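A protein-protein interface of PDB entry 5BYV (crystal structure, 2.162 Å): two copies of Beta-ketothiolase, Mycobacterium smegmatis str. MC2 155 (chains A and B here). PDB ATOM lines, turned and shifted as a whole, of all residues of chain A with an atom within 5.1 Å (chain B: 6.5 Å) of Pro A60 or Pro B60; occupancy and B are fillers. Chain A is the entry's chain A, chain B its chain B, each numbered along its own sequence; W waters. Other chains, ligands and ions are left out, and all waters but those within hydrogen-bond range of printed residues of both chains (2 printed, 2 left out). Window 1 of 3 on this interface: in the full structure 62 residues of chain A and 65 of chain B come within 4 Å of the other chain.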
ATOM      1  N   HIS A  57      -6.886  18.103   7.355  1.00  0.00           N
ATOM      2  CA  HIS A  57      -5.745  17.973   8.253  1.00  0.00           C
ATOM      3  C   HIS A  57      -4.782  19.047   7.806  1.00  0.00           C
ATOM      4  O   HIS A  57      -4.270  18.996   6.687  1.00  0.00           O
ATOM      5  CB  HIS A  57      -5.134  16.562   8.176  1.00  0.00           C
ATOM      6  CG  HIS A  57      -4.035  16.317   9.164  1.00  0.00           C
ATOM      7  ND1 HIS A  57      -4.097  16.747  10.473  1.00  0.00           N
ATOM      8  CD2 HIS A  57      -2.835  15.702   9.027  1.00  0.00           C
ATOM      9  CE1 HIS A  57      -2.986  16.398  11.101  1.00  0.00           C
ATOM     10  NE2 HIS A  57      -2.201  15.763  10.245  1.00  0.00           N
ATOM     11  N   CYS A  58      -4.566  20.035   8.665  1.00  0.00           N
ATOM     12  CA  CYS A  58      -3.942  21.275   8.225  1.00  0.00           C
ATOM     13  C   CYS A  58      -2.491  21.465   8.666  1.00  0.00           C
ATOM     14  O   CYS A  58      -1.799  22.348   8.165  1.00  0.00           O
ATOM     15  CB  CYS A  58      -4.795  22.453   8.690  1.00  0.00           C
ATOM     16  SG  CYS A  58      -6.438  22.416   7.973  1.00  0.00           S
ATOM     17  N   TYR A  59      -2.023  20.622   9.578  1.00  0.00           N
ATOM     18  CA  TYR A  59      -0.606  20.631   9.933  1.00  0.00           C
ATOM     19  C   TYR A  59      -0.008  19.257   9.780  1.00  0.00           C
ATOM     20  O   TYR A  59       0.595  18.745  10.716  1.00  0.00           O
ATOM     21  CB  TYR A  59      -0.413  21.143  11.366  1.00  0.00           C
ATOM     22  CG  TYR A  59      -0.897  22.565  11.487  1.00  0.00           C
ATOM     23  CD1 TYR A  59      -0.107  23.624  11.048  1.00  0.00           C
ATOM     24  CD2 TYR A  59      -2.167  22.847  11.983  1.00  0.00           C
ATOM     25  CE1 TYR A  59      -0.552  24.920  11.119  1.00  0.00           C
ATOM     26  CE2 TYR A  59      -2.619  24.139  12.064  1.00  0.00           C
ATOM     27  CZ  TYR A  59      -1.810  25.169  11.626  1.00  0.00           C
ATOM     28  OH  TYR A  59      -2.260  26.459  11.706  1.00  0.00           O
ATOM     29  N   PRO A  60      -0.161  18.655   8.591  1.00  0.00           N
ATOM     30  CA  PRO A  60       0.331  17.282   8.429  1.00  0.00           C
ATOM     31  C   PRO A  60       1.859  17.172   8.520  1.00  0.00           C
ATOM     32  O   PRO A  60       2.591  18.130   8.245  1.00  0.00           O
ATOM     33  CB  PRO A  60      -0.145  16.911   7.027  1.00  0.00           C
ATOM     34  CG  PRO A  60      -0.233  18.232   6.305  1.00  0.00           C
ATOM     35  CD  PRO A  60      -0.643  19.231   7.321  1.00  0.00           C
ATOM     36  N   ASN A  61       2.329  15.996   8.913  1.00  0.00           N
ATOM     37  CA  ASN A  61       3.748  15.711   8.907  1.00  0.00           C
ATOM     38  C   ASN A  61       3.943  14.219   8.780  1.00  0.00           C
ATOM     39  O   ASN A  61       2.979  13.466   8.825  1.00  0.00           O
ATOM     40  CB  ASN A  61       4.439  16.288  10.162  1.00  0.00           C
ATOM     41  CG  ASN A  61       3.903  15.713  11.479  1.00  0.00           C
ATOM     42  OD1 ASN A  61       3.832  14.503  11.670  1.00  0.00           O
ATOM     43  ND2 ASN A  61       3.528  16.600  12.393  1.00  0.00           N
ATOM     44  N   SER A  62       5.187  13.790   8.608  1.00  0.00           N
ATOM     45  CA  SER A  62       5.488  12.399   8.268  1.00  0.00           C
ATOM     46  C   SER A  62       5.221  11.399   9.377  1.00  0.00           C
ATOM     47  O   SER A  62       5.404  10.204   9.186  1.00  0.00           O
ATOM     48  CB  SER A  62       6.950  12.283   7.824  1.00  0.00           C
ATOM     49  OG  SER A  62       7.106  12.803   6.513  1.00  0.00           O
ATOM     50  N   GLN A  85      -5.508  12.782   2.770  1.00  0.00           N
ATOM     51  CA  GLN A  85      -5.477  14.027   3.532  1.00  0.00           C
ATOM     52  C   GLN A  85      -5.826  15.209   2.616  1.00  0.00           C
ATOM     53  O   GLN A  85      -5.387  15.247   1.467  1.00  0.00           O
ATOM     54  CB  GLN A  85      -4.081  14.214   4.174  1.00  0.00           C
ATOM     55  CG  GLN A  85      -3.858  15.541   4.905  1.00  0.00           C
ATOM     56  CD  GLN A  85      -3.208  16.604   4.045  1.00  0.00           C
ATOM     57  OE1 GLN A  85      -2.296  16.308   3.293  1.00  0.00           O
ATOM     58  NE2 GLN A  85      -3.651  17.853   4.178  1.00  0.00           N
ATOM     59  N   HIS B  57       0.551  17.098  -3.307  1.00  0.00           N
ATOM     60  CA  HIS B  57       1.677  17.668  -2.582  1.00  0.00           C
ATOM     61  C   HIS B  57       1.851  16.795  -1.348  1.00  0.00           C
ATOM     62  O   HIS B  57       0.970  16.763  -0.493  1.00  0.00           O
ATOM     63  CB  HIS B  57       1.378  19.138  -2.246  1.00  0.00           C
ATOM     64  CG  HIS B  57       2.524  19.892  -1.649  1.00  0.00           C
ATOM     65  ND1 HIS B  57       3.787  19.902  -2.193  1.00  0.00           N
ATOM     66  CD2 HIS B  57       2.582  20.681  -0.550  1.00  0.00           C
ATOM     67  CE1 HIS B  57       4.581  20.652  -1.446  1.00  0.00           C
ATOM     68  NE2 HIS B  57       3.875  21.131  -0.437  1.00  0.00           N
ATOM     69  N   CYS B  58       2.946  16.050  -1.266  1.00  0.00           N
ATOM     70  CA  CYS B  58       3.069  15.016  -0.230  1.00  0.00           C
ATOM     71  C   CYS B  58       3.919  15.393   0.972  1.00  0.00           C
ATOM     72  O   CYS B  58       3.849  14.751   2.017  1.00  0.00           O
ATOM     73  CB  CYS B  58       3.625  13.740  -0.845  1.00  0.00           C
ATOM     74  SG  CYS B  58       2.644  13.229  -2.242  1.00  0.00           S
ATOM     75  N   TYR B  59       4.696  16.455   0.847  1.00  0.00           N
ATOM     76  CA  TYR B  59       5.454  16.914   1.988  1.00  0.00           C
ATOM     77  C   TYR B  59       5.133  18.354   2.308  1.00  0.00           C
ATOM     78  O   TYR B  59       6.029  19.201   2.278  1.00  0.00           O
ATOM     79  CB  TYR B  59       6.946  16.724   1.722  1.00  0.00           C
ATOM     80  CG  TYR B  59       7.254  15.284   1.406  1.00  0.00           C
ATOM     81  CD1 TYR B  59       7.348  14.341   2.417  1.00  0.00           C
ATOM     82  CD2 TYR B  59       7.402  14.856   0.098  1.00  0.00           C
ATOM     83  CE1 TYR B  59       7.610  13.018   2.140  1.00  0.00           C
ATOM     84  CE2 TYR B  59       7.663  13.530  -0.189  1.00  0.00           C
ATOM     85  CZ  TYR B  59       7.770  12.621   0.836  1.00  0.00           C
ATOM     86  OH  TYR B  59       8.043  11.308   0.556  1.00  0.00           O
ATOM     87  N   PRO B  60       3.849  18.644   2.612  1.00  0.00           N
ATOM     88  CA  PRO B  60       3.511  20.034   2.926  1.00  0.00           C
ATOM     89  C   PRO B  60       4.115  20.529   4.247  1.00  0.00           C
ATOM     90  O   PRO B  60       4.370  19.749   5.173  1.00  0.00           O
ATOM     91  CB  PRO B  60       1.982  20.001   3.017  1.00  0.00           C
ATOM     92  CG  PRO B  60       1.655  18.597   3.359  1.00  0.00           C
ATOM     93  CD  PRO B  60       2.659  17.770   2.655  1.00  0.00           C
ATOM     94  N   ASN B  61       4.351  21.833   4.330  1.00  0.00           N
ATOM     95  CA  ASN B  61       4.686  22.459   5.603  1.00  0.00           C
ATOM     96  C   ASN B  61       4.225  23.917   5.595  1.00  0.00           C
ATOM     97  O   ASN B  61       3.672  24.390   4.595  1.00  0.00           O
ATOM     98  CB  ASN B  61       6.199  22.318   5.912  1.00  0.00           C
ATOM     99  CG  ASN B  61       7.098  22.922   4.837  1.00  0.00           C
ATOM    100  OD1 ASN B  61       6.907  24.060   4.425  1.00  0.00           O
ATOM    101  ND2 ASN B  61       8.090  22.157   4.387  1.00  0.00           N
ATOM    102  N   SER B  62       4.441  24.626   6.698  1.00  0.00           N
ATOM    103  CA  SER B  62       3.932  25.979   6.849  1.00  0.00           C
ATOM    104  C   SER B  62       4.616  27.015   5.976  1.00  0.00           C
ATOM    105  O   SER B  62       4.289  28.197   6.040  1.00  0.00           O
ATOM    106  CB  SER B  62       4.050  26.394   8.302  1.00  0.00           C
ATOM    107  OG  SER B  62       3.093  25.701   9.080  1.00  0.00           O
ATOM    108  N   GLU B  63       5.567  26.592   5.162  1.00  0.00           N
ATOM    109  CA  GLU B  63       6.149  27.501   4.183  1.00  0.00           C
ATOM    110  C   GLU B  63       5.091  27.840   3.131  1.00  0.00           C
ATOM    111  O   GLU B  63       5.084  28.927   2.562  1.00  0.00           O
ATOM    112  CB  GLU B  63       7.385  26.880   3.534  1.00  0.00           C
ATOM    113  CG  GLU B  63       8.546  26.662   4.502  1.00  0.00           C
ATOM    114  CD  GLU B  63       8.889  27.927   5.252  1.00  0.00           C
ATOM    115  OE1 GLU B  63       9.287  28.890   4.569  1.00  0.00           O
ATOM    116  OE2 GLU B  63       8.761  27.975   6.501  1.00  0.00           O
ATOM    117  N   ALA B  64       4.179  26.898   2.903  1.00  0.00           N
ATOM    118  CA  ALA B  64       3.096  27.064   1.932  1.00  0.00           C
ATOM    119  C   ALA B  64       1.868  26.249   2.314  1.00  0.00           C
ATOM    120  O   ALA B  64       1.704  25.125   1.848  1.00  0.00           O
ATOM    121  CB  ALA B  64       3.566  26.677   0.565  1.00  0.00           C
ATOM    122  N   ILE B  67      -1.352  24.595  -0.569  1.00  0.00           N
ATOM    123  CA  ILE B  67      -0.364  25.083  -1.527  1.00  0.00           C
ATOM    124  C   ILE B  67      -0.949  25.564  -2.845  1.00  0.00           C
ATOM    125  O   ILE B  67      -0.406  26.473  -3.445  1.00  0.00           O
ATOM    126  CB  ILE B  67       0.734  24.026  -1.809  1.00  0.00           C
ATOM    127  CG1 ILE B  67       1.871  24.658  -2.623  1.00  0.00           C
ATOM    128  CG2 ILE B  67       0.161  22.755  -2.443  1.00  0.00           C
ATOM    129  CD1 ILE B  67       3.166  23.858  -2.664  1.00  0.00           C
ATOM    130  N   GLN B  85      -4.629  21.748  -1.129  1.00  0.00           N
ATOM    131  CA  GLN B  85      -3.581  20.735  -1.181  1.00  0.00           C
ATOM    132  C   GLN B  85      -4.230  19.393  -0.894  1.00  0.00           C
ATOM    133  O   GLN B  85      -5.115  19.323  -0.053  1.00  0.00           O
ATOM    134  CB  GLN B  85      -2.465  21.056  -0.157  1.00  0.00           C
ATOM    135  CG  GLN B  85      -1.330  20.019  -0.018  1.00  0.00           C
ATOM    136  CD  GLN B  85      -1.556  18.997   1.101  1.00  0.00           C
ATOM    137  OE1 GLN B  85      -2.040  19.346   2.174  1.00  0.00           O
ATOM    138  NE2 GLN B  85      -1.157  17.747   0.870  1.00  0.00           N
ATOM    139  N   ASP B  87      -3.219  15.003  -0.410  1.00  0.00           N
ATOM    140  CA  ASP B  87      -2.128  14.049  -0.266  1.00  0.00           C
ATOM    141  C   ASP B  87      -2.660  12.633  -0.187  1.00  0.00           C
ATOM    142  O   ASP B  87      -3.292  12.245   0.784  1.00  0.00           O
ATOM    143  CB  ASP B  87      -1.273  14.370   0.976  1.00  0.00           C
ATOM    144  CG  ASP B  87      -0.251  13.267   1.304  1.00  0.00           C
ATOM    145  OD1 ASP B  87       0.200  12.537   0.392  1.00  0.00           O
ATOM    146  OD2 ASP B  87       0.142  13.148   2.479  1.00  0.00           O
ATOM    147  N   ARG B  89      -0.212  10.306  -1.038  1.00  0.00           N
ATOM    148  CA  ARG B  89       1.184  10.005  -1.405  1.00  0.00           C
ATOM    149  C   ARG B  89       1.477  10.081  -2.901  1.00  0.00           C
ATOM    150  O   ARG B  89       1.144  11.064  -3.578  1.00  0.00           O
ATOM    151  CB  ARG B  89       1.583   8.620  -0.891  1.00  0.00           C
ATOM    152  CG  ARG B  89       1.431   8.444   0.597  1.00  0.00           C
ATOM    153  CD  ARG B  89       2.645   8.996   1.324  1.00  0.00           C
ATOM    154  NE  ARG B  89       2.428  10.360   1.766  1.00  0.00           N
ATOM    155  CZ  ARG B  89       3.385  11.210   2.130  1.00  0.00           C
ATOM    156  NH1 ARG B  89       4.663  10.855   2.131  1.00  0.00           N
ATOM    157  NH2 ARG B  89       3.044  12.421   2.519  1.00  0.00           N
ATOM    158  N   GLU B 118       6.387  19.238  -6.087  1.00  0.00           N
ATOM    159  CA  GLU B 118       7.221  18.653  -5.054  1.00  0.00           C
ATOM    160  C   GLU B 118       8.648  19.104  -5.202  1.00  0.00           C
ATOM    161  O   GLU B 118       9.230  18.982  -6.276  1.00  0.00           O
ATOM    162  CB  GLU B 118       7.172  17.132  -5.093  1.00  0.00           C
ATOM    163  CG  GLU B 118       7.329  16.505  -3.735  1.00  0.00           C
ATOM    164  CD  GLU B 118       6.074  16.655  -2.913  1.00  0.00           C
ATOM    165  OE1 GLU B 118       6.091  17.367  -1.878  1.00  0.00           O
ATOM    166  OE2 GLU B 118       5.048  16.066  -3.301  1.00  0.00           O
HETATM  167  O   HOH W   1      -0.025  14.901   4.299  1.00  0.00           O
HETATM  168  O   HOH W   2       4.739  19.256   7.790  1.00  0.00           O
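The side-chain sulfur (SG) of Cys B58 sits at hydrogen-bond distance from the side-chain carboxylate (OD1) of Asp B87 (3.7 Å). The backbone carbonyl oxygen (O) of His A57 is in hydrogen-bond range of the side-chain amide nitrogen (NE2) of Gln A85 (2.8 Å). The side-chain amide nitrogen of Gln B85 lies within hydrogen-bond range of the backbone carbonyl oxygen of His B57 (2.7 Å). OD2 of Asp B87 is in salt-bridge range of NH2 of Arg B89 (3.0 Å).
The side-chain amide nitrogen (NE2) of Gln A85 is in hydrogen-bond range of the side-chain amide oxygen (OE1) of Gln B85. The backbone NH of Asp B87 sits at hydrogen-bond distance from the backbone carbonyl oxygen of Gln A85 (2.9 Å).
Pro A60 touches its own counterpart, Pro B60. Gln B85 touches its own counterpart, Gln A85. Of the 3 pairs that touch across the chains among the printed residues, 2 have their exchanged pair printed and touching as well.
Hydrophobic or aromatic side chains of chain A that line the printed part of chain B: Pro A60. Printed residues of chain B that touch a printed residue of chain A: Pro B60, Gln B85 and Asp B87. Hydrophobic or aromatic side chains of chain B that line the printed part of chain A: Pro B60.
Pro A60 touches just one residue of chain B: Pro B60. Pro B60 touches just one residue of chain A: Pro A60 (3.5 Å). Of the printed residues of chain B, Gln A85 touches Gln B85 (3.0 Å) and Asp B87 (2.9 Å). Printed residues of chain A within 4 Å of Asp B87: Gln A85 (2.9 Å). Glu B63 touches none of the printed residues of chain A. The nearest residue of chain B that does not touch Pro A60 is Gln B85 (4.6 Å). The nearest residue of chain A that does not touch Pro B60 is Gln A85 (4.6 Å).
Pro A60 touches Pro B60 (CG to CG, 3.5 Å).
Water W2 bridges O of Pro A60 (2.5 Å) and O of Pro B60 (2.7 Å). Water W1 bridges OD2 of Asp B87 (2.5 Å) and OE1 of Gln A85 (2.9 Å).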
